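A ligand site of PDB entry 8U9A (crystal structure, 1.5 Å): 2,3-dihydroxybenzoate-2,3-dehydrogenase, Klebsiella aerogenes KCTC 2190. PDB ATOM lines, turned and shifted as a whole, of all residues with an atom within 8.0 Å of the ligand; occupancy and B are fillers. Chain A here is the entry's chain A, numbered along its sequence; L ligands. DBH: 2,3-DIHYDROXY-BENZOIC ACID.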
ATOM      1  N   ASP A 143      19.010  19.857   5.779  1.00  0.00           N
ATOM      2  CA  ASP A 143      20.072  18.866   5.963  1.00  0.00           C
ATOM      3  C   ASP A 143      21.166  19.393   6.868  1.00  0.00           C
ATOM      4  O   ASP A 143      21.936  18.602   7.419  1.00  0.00           O
ATOM      5  CB  ASP A 143      20.615  18.340   4.623  1.00  0.00           C
ATOM      6  CG  ASP A 143      21.334  19.384   3.770  1.00  0.00           C
ATOM      7  OD1 ASP A 143      21.465  20.561   4.161  1.00  0.00           O
ATOM      8  OD2 ASP A 143      21.768  18.964   2.663  1.00  0.00           O
ATOM      9  N   ARG A 149      27.859  21.895   9.133  1.00  0.00           N
ATOM     10  CA  ARG A 149      28.179  22.584   7.878  1.00  0.00           C
ATOM     11  C   ARG A 149      28.885  23.887   8.203  1.00  0.00           C
ATOM     12  O   ARG A 149      28.300  24.750   8.858  1.00  0.00           O
ATOM     13  CB  ARG A 149      26.901  22.850   7.089  1.00  0.00           C
ATOM     14  CG  ARG A 149      26.208  21.561   6.633  1.00  0.00           C
ATOM     15  CD  ARG A 149      26.849  20.999   5.389  1.00  0.00           C
ATOM     16  NE  ARG A 149      26.612  21.868   4.253  1.00  0.00           N
ATOM     17  CZ  ARG A 149      25.479  21.916   3.558  1.00  0.00           C
ATOM     18  NH1 ARG A 149      24.471  21.094   3.841  1.00  0.00           N
ATOM     19  NH2 ARG A 149      25.352  22.798   2.570  1.00  0.00           N
ATOM     20  N   SER A 184      13.794  17.734   5.047  1.00  0.00           N
ATOM     21  CA  SER A 184      15.061  18.426   5.262  1.00  0.00           C
ATOM     22  C   SER A 184      15.698  18.714   3.907  1.00  0.00           C
ATOM     23  O   SER A 184      16.411  17.852   3.351  1.00  0.00           O
ATOM     24  CB  SER A 184      15.989  17.577   6.137  1.00  0.00           C
ATOM     25  OG  SER A 184      15.565  17.628   7.488  1.00  0.00           O
ATOM     26  N   PRO A 185      15.451  19.875   3.334  1.00  0.00           N
ATOM     27  CA  PRO A 185      16.050  20.210   2.041  1.00  0.00           C
ATOM     28  C   PRO A 185      17.530  20.521   2.167  1.00  0.00           C
ATOM     29  O   PRO A 185      18.047  20.839   3.230  1.00  0.00           O
ATOM     30  CB  PRO A 185      15.283  21.460   1.594  1.00  0.00           C
ATOM     31  CG  PRO A 185      14.111  21.556   2.501  1.00  0.00           C
ATOM     32  CD  PRO A 185      14.515  20.909   3.799  1.00  0.00           C
ATOM     33  N   GLY A 186      18.198  20.491   1.013  1.00  0.00           N
ATOM     34  CA  GLY A 186      19.543  20.972   0.910  1.00  0.00           C
ATOM     35  C   GLY A 186      19.693  22.464   1.135  1.00  0.00           C
ATOM     36  O   GLY A 186      18.733  23.216   1.309  1.00  0.00           O
ATOM     37  N   SER A 187      20.945  22.902   1.112  1.00  0.00           N
ATOM     38  CA  SER A 187      21.287  24.273   1.452  1.00  0.00           C
ATOM     39  C   SER A 187      22.375  24.818   0.533  1.00  0.00           C
ATOM     40  O   SER A 187      22.356  24.572  -0.669  1.00  0.00           O
ATOM     41  CB  SER A 187      21.741  24.350   2.916  1.00  0.00           C
ATOM     42  OG  SER A 187      22.667  23.308   3.208  1.00  0.00           O
ATOM     43  N   GLY A 217      29.886  10.683  -7.024  1.00  0.00           N
ATOM     44  CA  GLY A 217      28.692  11.197  -7.676  1.00  0.00           C
ATOM     45  C   GLY A 217      27.623  11.726  -6.729  1.00  0.00           C
ATOM     46  O   GLY A 217      26.442  11.773  -7.065  1.00  0.00           O
ATOM     47  N   ILE A 218      28.037  12.129  -5.530  1.00  0.00           N
ATOM     48  CA  ILE A 218      27.132  12.748  -4.569  1.00  0.00           C
ATOM     49  C   ILE A 218      27.547  14.212  -4.439  1.00  0.00           C
ATOM     50  O   ILE A 218      28.744  14.502  -4.337  1.00  0.00           O
ATOM     51  CB  ILE A 218      27.149  12.015  -3.223  1.00  0.00           C
ATOM     52  CG1 ILE A 218      26.559  10.603  -3.350  1.00  0.00           C
ATOM     53  CG2 ILE A 218      26.396  12.820  -2.163  1.00  0.00           C
ATOM     54  CD1 ILE A 218      25.050  10.581  -3.494  1.00  0.00           C
ATOM     55  N   PRO A 219      26.595  15.172  -4.436  1.00  0.00           N
ATOM     56  CA  PRO A 219      25.143  14.988  -4.545  1.00  0.00           C
ATOM     57  C   PRO A 219      24.718  14.538  -5.931  1.00  0.00           C
ATOM     58  O   PRO A 219      25.340  14.838  -6.946  1.00  0.00           O
ATOM     59  CB  PRO A 219      24.599  16.374  -4.184  1.00  0.00           C
ATOM     60  CG  PRO A 219      25.693  17.326  -4.555  1.00  0.00           C
ATOM     61  CD  PRO A 219      26.968  16.586  -4.239  1.00  0.00           C
ATOM     62  N   LEU A 220      23.624  13.777  -5.944  1.00  0.00           N
ATOM     63  CA  LEU A 220      23.067  13.205  -7.163  1.00  0.00           C
ATOM     64  C   LEU A 220      21.966  14.119  -7.682  1.00  0.00           C
ATOM     65  O   LEU A 220      20.988  14.390  -6.972  1.00  0.00           O
ATOM     66  CB  LEU A 220      22.519  11.808  -6.863  1.00  0.00           C
ATOM     67  CG  LEU A 220      21.930  11.007  -8.020  1.00  0.00           C
ATOM     68  CD1 LEU A 220      22.987  10.839  -9.065  1.00  0.00           C
ATOM     69  CD2 LEU A 220      21.435   9.660  -7.521  1.00  0.00           C
ATOM     70  N   GLY A 221      22.135  14.604  -8.923  1.00  0.00           N
ATOM     71  CA  GLY A 221      21.146  15.459  -9.556  1.00  0.00           C
ATOM     72  C   GLY A 221      21.390  16.947  -9.299  1.00  0.00           C
ATOM     73  O   GLY A 221      22.314  17.351  -8.597  1.00  0.00           O
ATOM     74  N   LYS A 222      20.529  17.760  -9.898  1.00  0.00           N
ATOM     75  CA  LYS A 222      20.589  19.197  -9.688  1.00  0.00           C
ATOM     76  C   LYS A 222      19.902  19.568  -8.377  1.00  0.00           C
ATOM     77  O   LYS A 222      19.133  18.788  -7.801  1.00  0.00           O
ATOM     78  CB  LYS A 222      19.928  19.944 -10.846  1.00  0.00           C
ATOM     79  CG  LYS A 222      20.596  19.688 -12.192  1.00  0.00           C
ATOM     80  CD  LYS A 222      20.558  20.912 -13.096  1.00  0.00           C
ATOM     81  CE  LYS A 222      21.297  20.656 -14.401  1.00  0.00           C
ATOM     82  NZ  LYS A 222      21.481  21.916 -15.198  1.00  0.00           N
ATOM     83  N   ILE A 223      20.174  20.798  -7.908  1.00  0.00           N
ATOM     84  CA  ILE A 223      19.568  21.281  -6.669  1.00  0.00           C
ATOM     85  C   ILE A 223      18.056  21.147  -6.766  1.00  0.00           C
ATOM     86  O   ILE A 223      17.454  21.430  -7.817  1.00  0.00           O
ATOM     87  CB  ILE A 223      19.968  22.737  -6.392  1.00  0.00           C
ATOM     88  CG1 ILE A 223      21.487  22.970  -6.523  1.00  0.00           C
ATOM     89  CG2 ILE A 223      19.462  23.172  -5.016  1.00  0.00           C
ATOM     90  CD1 ILE A 223      22.342  22.233  -5.512  1.00  0.00           C
ATOM     91  N   ALA A 224      17.428  20.713  -5.675  1.00  0.00           N
ATOM     92  CA  ALA A 224      15.976  20.559  -5.648  1.00  0.00           C
ATOM     93  C   ALA A 224      15.297  21.918  -5.602  1.00  0.00           C
ATOM     94  O   ALA A 224      15.626  22.757  -4.763  1.00  0.00           O
ATOM     95  CB  ALA A 224      15.552  19.731  -4.447  1.00  0.00           C
ATOM     96  N   ARG A 225      14.346  22.133  -6.510  1.00  0.00           N
ATOM     97  CA  ARG A 225      13.611  23.376  -6.566  1.00  0.00           C
ATOM     98  C   ARG A 225      12.472  23.356  -5.549  1.00  0.00           C
ATOM     99  O   ARG A 225      12.031  22.285  -5.141  1.00  0.00           O
ATOM    100  CB  ARG A 225      13.056  23.582  -7.971  1.00  0.00           C
ATOM    101  CG  ARG A 225      14.129  23.652  -9.044  1.00  0.00           C
ATOM    102  CD  ARG A 225      13.509  23.737 -10.411  1.00  0.00           C
ATOM    103  NE  ARG A 225      14.514  23.980 -11.431  1.00  0.00           N
ATOM    104  CZ  ARG A 225      14.238  24.224 -12.702  1.00  0.00           C
ATOM    105  NH1 ARG A 225      12.987  24.271 -13.139  1.00  0.00           N
ATOM    106  NH2 ARG A 225      15.235  24.422 -13.559  1.00  0.00           N
ATOM    107  N   GLU A 228       9.664  20.960  -6.080  1.00  0.00           N
ATOM    108  CA  GLU A 228       9.932  19.545  -5.858  1.00  0.00           C
ATOM    109  C   GLU A 228       9.901  19.193  -4.364  1.00  0.00           C
ATOM    110  O   GLU A 228       9.414  18.133  -3.980  1.00  0.00           O
ATOM    111  CB  GLU A 228      11.278  19.166  -6.493  1.00  0.00           C
ATOM    112  CG  GLU A 228      11.353  19.553  -7.970  1.00  0.00           C
ATOM    113  CD  GLU A 228      12.701  19.250  -8.610  1.00  0.00           C
ATOM    114  OE1 GLU A 228      13.640  20.063  -8.454  1.00  0.00           O
ATOM    115  OE2 GLU A 228      12.825  18.197  -9.299  1.00  0.00           O
ATOM    116  N   ILE A 229      10.405  20.088  -3.500  1.00  0.00           N
ATOM    117  CA  ILE A 229      10.261  19.896  -2.068  1.00  0.00           C
ATOM    118  C   ILE A 229       8.787  19.874  -1.678  1.00  0.00           C
ATOM    119  O   ILE A 229       8.359  19.058  -0.838  1.00  0.00           O
ATOM    120  CB  ILE A 229      11.009  21.011  -1.315  1.00  0.00           C
ATOM    121  CG1 ILE A 229      12.493  21.010  -1.661  1.00  0.00           C
ATOM    122  CG2 ILE A 229      10.790  20.908   0.164  1.00  0.00           C
ATOM    123  CD1 ILE A 229      13.209  19.804  -1.213  1.00  0.00           C
ATOM    124  N   VAL A 250      15.220  13.554   3.987  1.00  0.00           N
ATOM    125  CA  VAL A 250      16.263  14.481   3.536  1.00  0.00           C
ATOM    126  C   VAL A 250      16.245  14.501   2.018  1.00  0.00           C
ATOM    127  O   VAL A 250      16.413  13.478   1.359  1.00  0.00           O
ATOM    128  CB  VAL A 250      17.642  14.068   4.049  1.00  0.00           C
ATOM    129  CG1 VAL A 250      18.659  15.099   3.626  1.00  0.00           C
ATOM    130  CG2 VAL A 250      17.659  13.972   5.572  1.00  0.00           C
ATOM    131  N   VAL A 251      16.065  15.689   1.466  1.00  0.00           N
ATOM    132  CA  VAL A 251      15.924  15.873   0.029  1.00  0.00           C
ATOM    133  C   VAL A 251      17.059  16.763  -0.423  1.00  0.00           C
ATOM    134  O   VAL A 251      16.911  17.977  -0.551  1.00  0.00           O
ATOM    135  CB  VAL A 251      14.568  16.502  -0.319  1.00  0.00           C
ATOM    136  CG1 VAL A 251      14.413  16.607  -1.811  1.00  0.00           C
ATOM    137  CG2 VAL A 251      13.412  15.681   0.268  1.00  0.00           C
ATOM    138  N   ASP A 252      18.237  16.164  -0.616  1.00  0.00           N
ATOM    139  CA  ASP A 252      19.437  16.920  -0.950  1.00  0.00           C
ATOM    140  C   ASP A 252      20.368  16.110  -1.834  1.00  0.00           C
ATOM    141  O   ASP A 252      21.572  16.369  -1.861  1.00  0.00           O
ATOM    142  CB  ASP A 252      20.159  17.406   0.330  1.00  0.00           C
ATOM    143  CG  ASP A 252      20.722  16.261   1.154  1.00  0.00           C
ATOM    144  OD1 ASP A 252      20.492  15.113   0.784  1.00  0.00           O
ATOM    145  OD2 ASP A 252      21.428  16.532   2.171  1.00  0.00           O
ATOM    146  N   GLY A 253      19.823  15.146  -2.577  1.00  0.00           N
ATOM    147  CA  GLY A 253      20.658  14.395  -3.496  1.00  0.00           C
ATOM    148  C   GLY A 253      21.629  13.476  -2.809  1.00  0.00           C
ATOM    149  O   GLY A 253      22.616  13.056  -3.419  1.00  0.00           O
ATOM    150  N   GLY A 254      21.376  13.139  -1.546  1.00  0.00           N
ATOM    151  CA  GLY A 254      22.214  12.195  -0.824  1.00  0.00           C
ATOM    152  C   GLY A 254      23.411  12.803  -0.135  1.00  0.00           C
ATOM    153  O   GLY A 254      24.278  12.045   0.303  1.00  0.00           O
ATOM    154  N   SER A 255      23.464  14.123   0.008  1.00  0.00           N
ATOM    155  CA  SER A 255      24.673  14.802   0.489  1.00  0.00           C
ATOM    156  C   SER A 255      25.038  14.408   1.908  1.00  0.00           C
ATOM    157  O   SER A 255      26.221  14.469   2.271  1.00  0.00           O
ATOM    158  CB  SER A 255      24.472  16.315   0.430  1.00  0.00           C
ATOM    159  OG  SER A 255      24.502  16.737  -0.922  1.00  0.00           O
HETATM  160  O17 DBH L   1      18.800  20.181  -2.618  1.00  0.00           O
HETATM  161  C21 DBH L   1      20.013  20.200  -2.850  1.00  0.00           C
HETATM  162  O9  DBH L   1      20.865  20.988  -2.311  1.00  0.00           O
HETATM  163  C18 DBH L   1      20.572  19.230  -3.873  1.00  0.00           C
HETATM  164  C15 DBH L   1      21.883  19.362  -4.296  1.00  0.00           C
HETATM  165  C12 DBH L   1      22.406  18.511  -5.249  1.00  0.00           C
HETATM  166  C3  DBH L   1      19.761  18.215  -4.413  1.00  0.00           C
HETATM  167  O3  DBH L   1      18.487  18.035  -4.052  1.00  0.00           O
HETATM  168  C6  DBH L   1      20.302  17.339  -5.375  1.00  0.00           C
HETATM  169  C9  DBH L   1      21.609  17.494  -5.775  1.00  0.00           C
HETATM  170  O6  DBH L   1      19.467  16.373  -5.854  1.00  0.00           O
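An oxygen (O6) of the ligand is in hydrogen-bond range of the backbone carbonyl oxygen of Leu 220.
O of Lys 222 lies close to O6 of the ligand (3.1 Å).
O3 of the ligand sits at hydrogen-bond distance from N of Ala 224 (3.3 Å).
The backbone NH of Leu 220 lies within hydrogen-bond range of the backbone carbonyl oxygen of Gly 253 (2.8 Å).
O of Asp 252 lies within hydrogen-bond range of OG of Ser 255 (3.1 Å).
The side-chain carboxylate (OD2) of Asp 252 sits close to the side-chain carboxylate (OD2) of Asp 143 (2.5 Å).
OD1 of Asp 252 lies close to N of Gly 254, 3.2 Å away.
O of Val 251 is in hydrogen-bond range of N of Gly 186 (3.2 Å).
The backbone NH (N) of Val 251 is in hydrogen-bond range of the backbone carbonyl oxygen (O) of Ser 184 (2.9 Å).
OG of Ser 187 sits at hydrogen-bond distance from OD1 of Asp 143.
OG of Ser 187 is in hydrogen-bond range of NH2 of Arg 149, at 2.8 Å.
Merely in contact with the ligand: Gly 186, Ser 187, Pro 219, Gly 221, Ile 223, Val 251, Asp 252 and Gly 253.
Hydrophobic or aromatic side chains that line the ligand: Pro 219, Ile 223 and Ala 224.
11 residues have an atom within 4 Å of the ligand: Gly 186, Ser 187, Pro 219, Leu 220, Gly 221, Lys 222, Ile 223, Ala 224, Val 251, Asp 252 and Gly 253.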
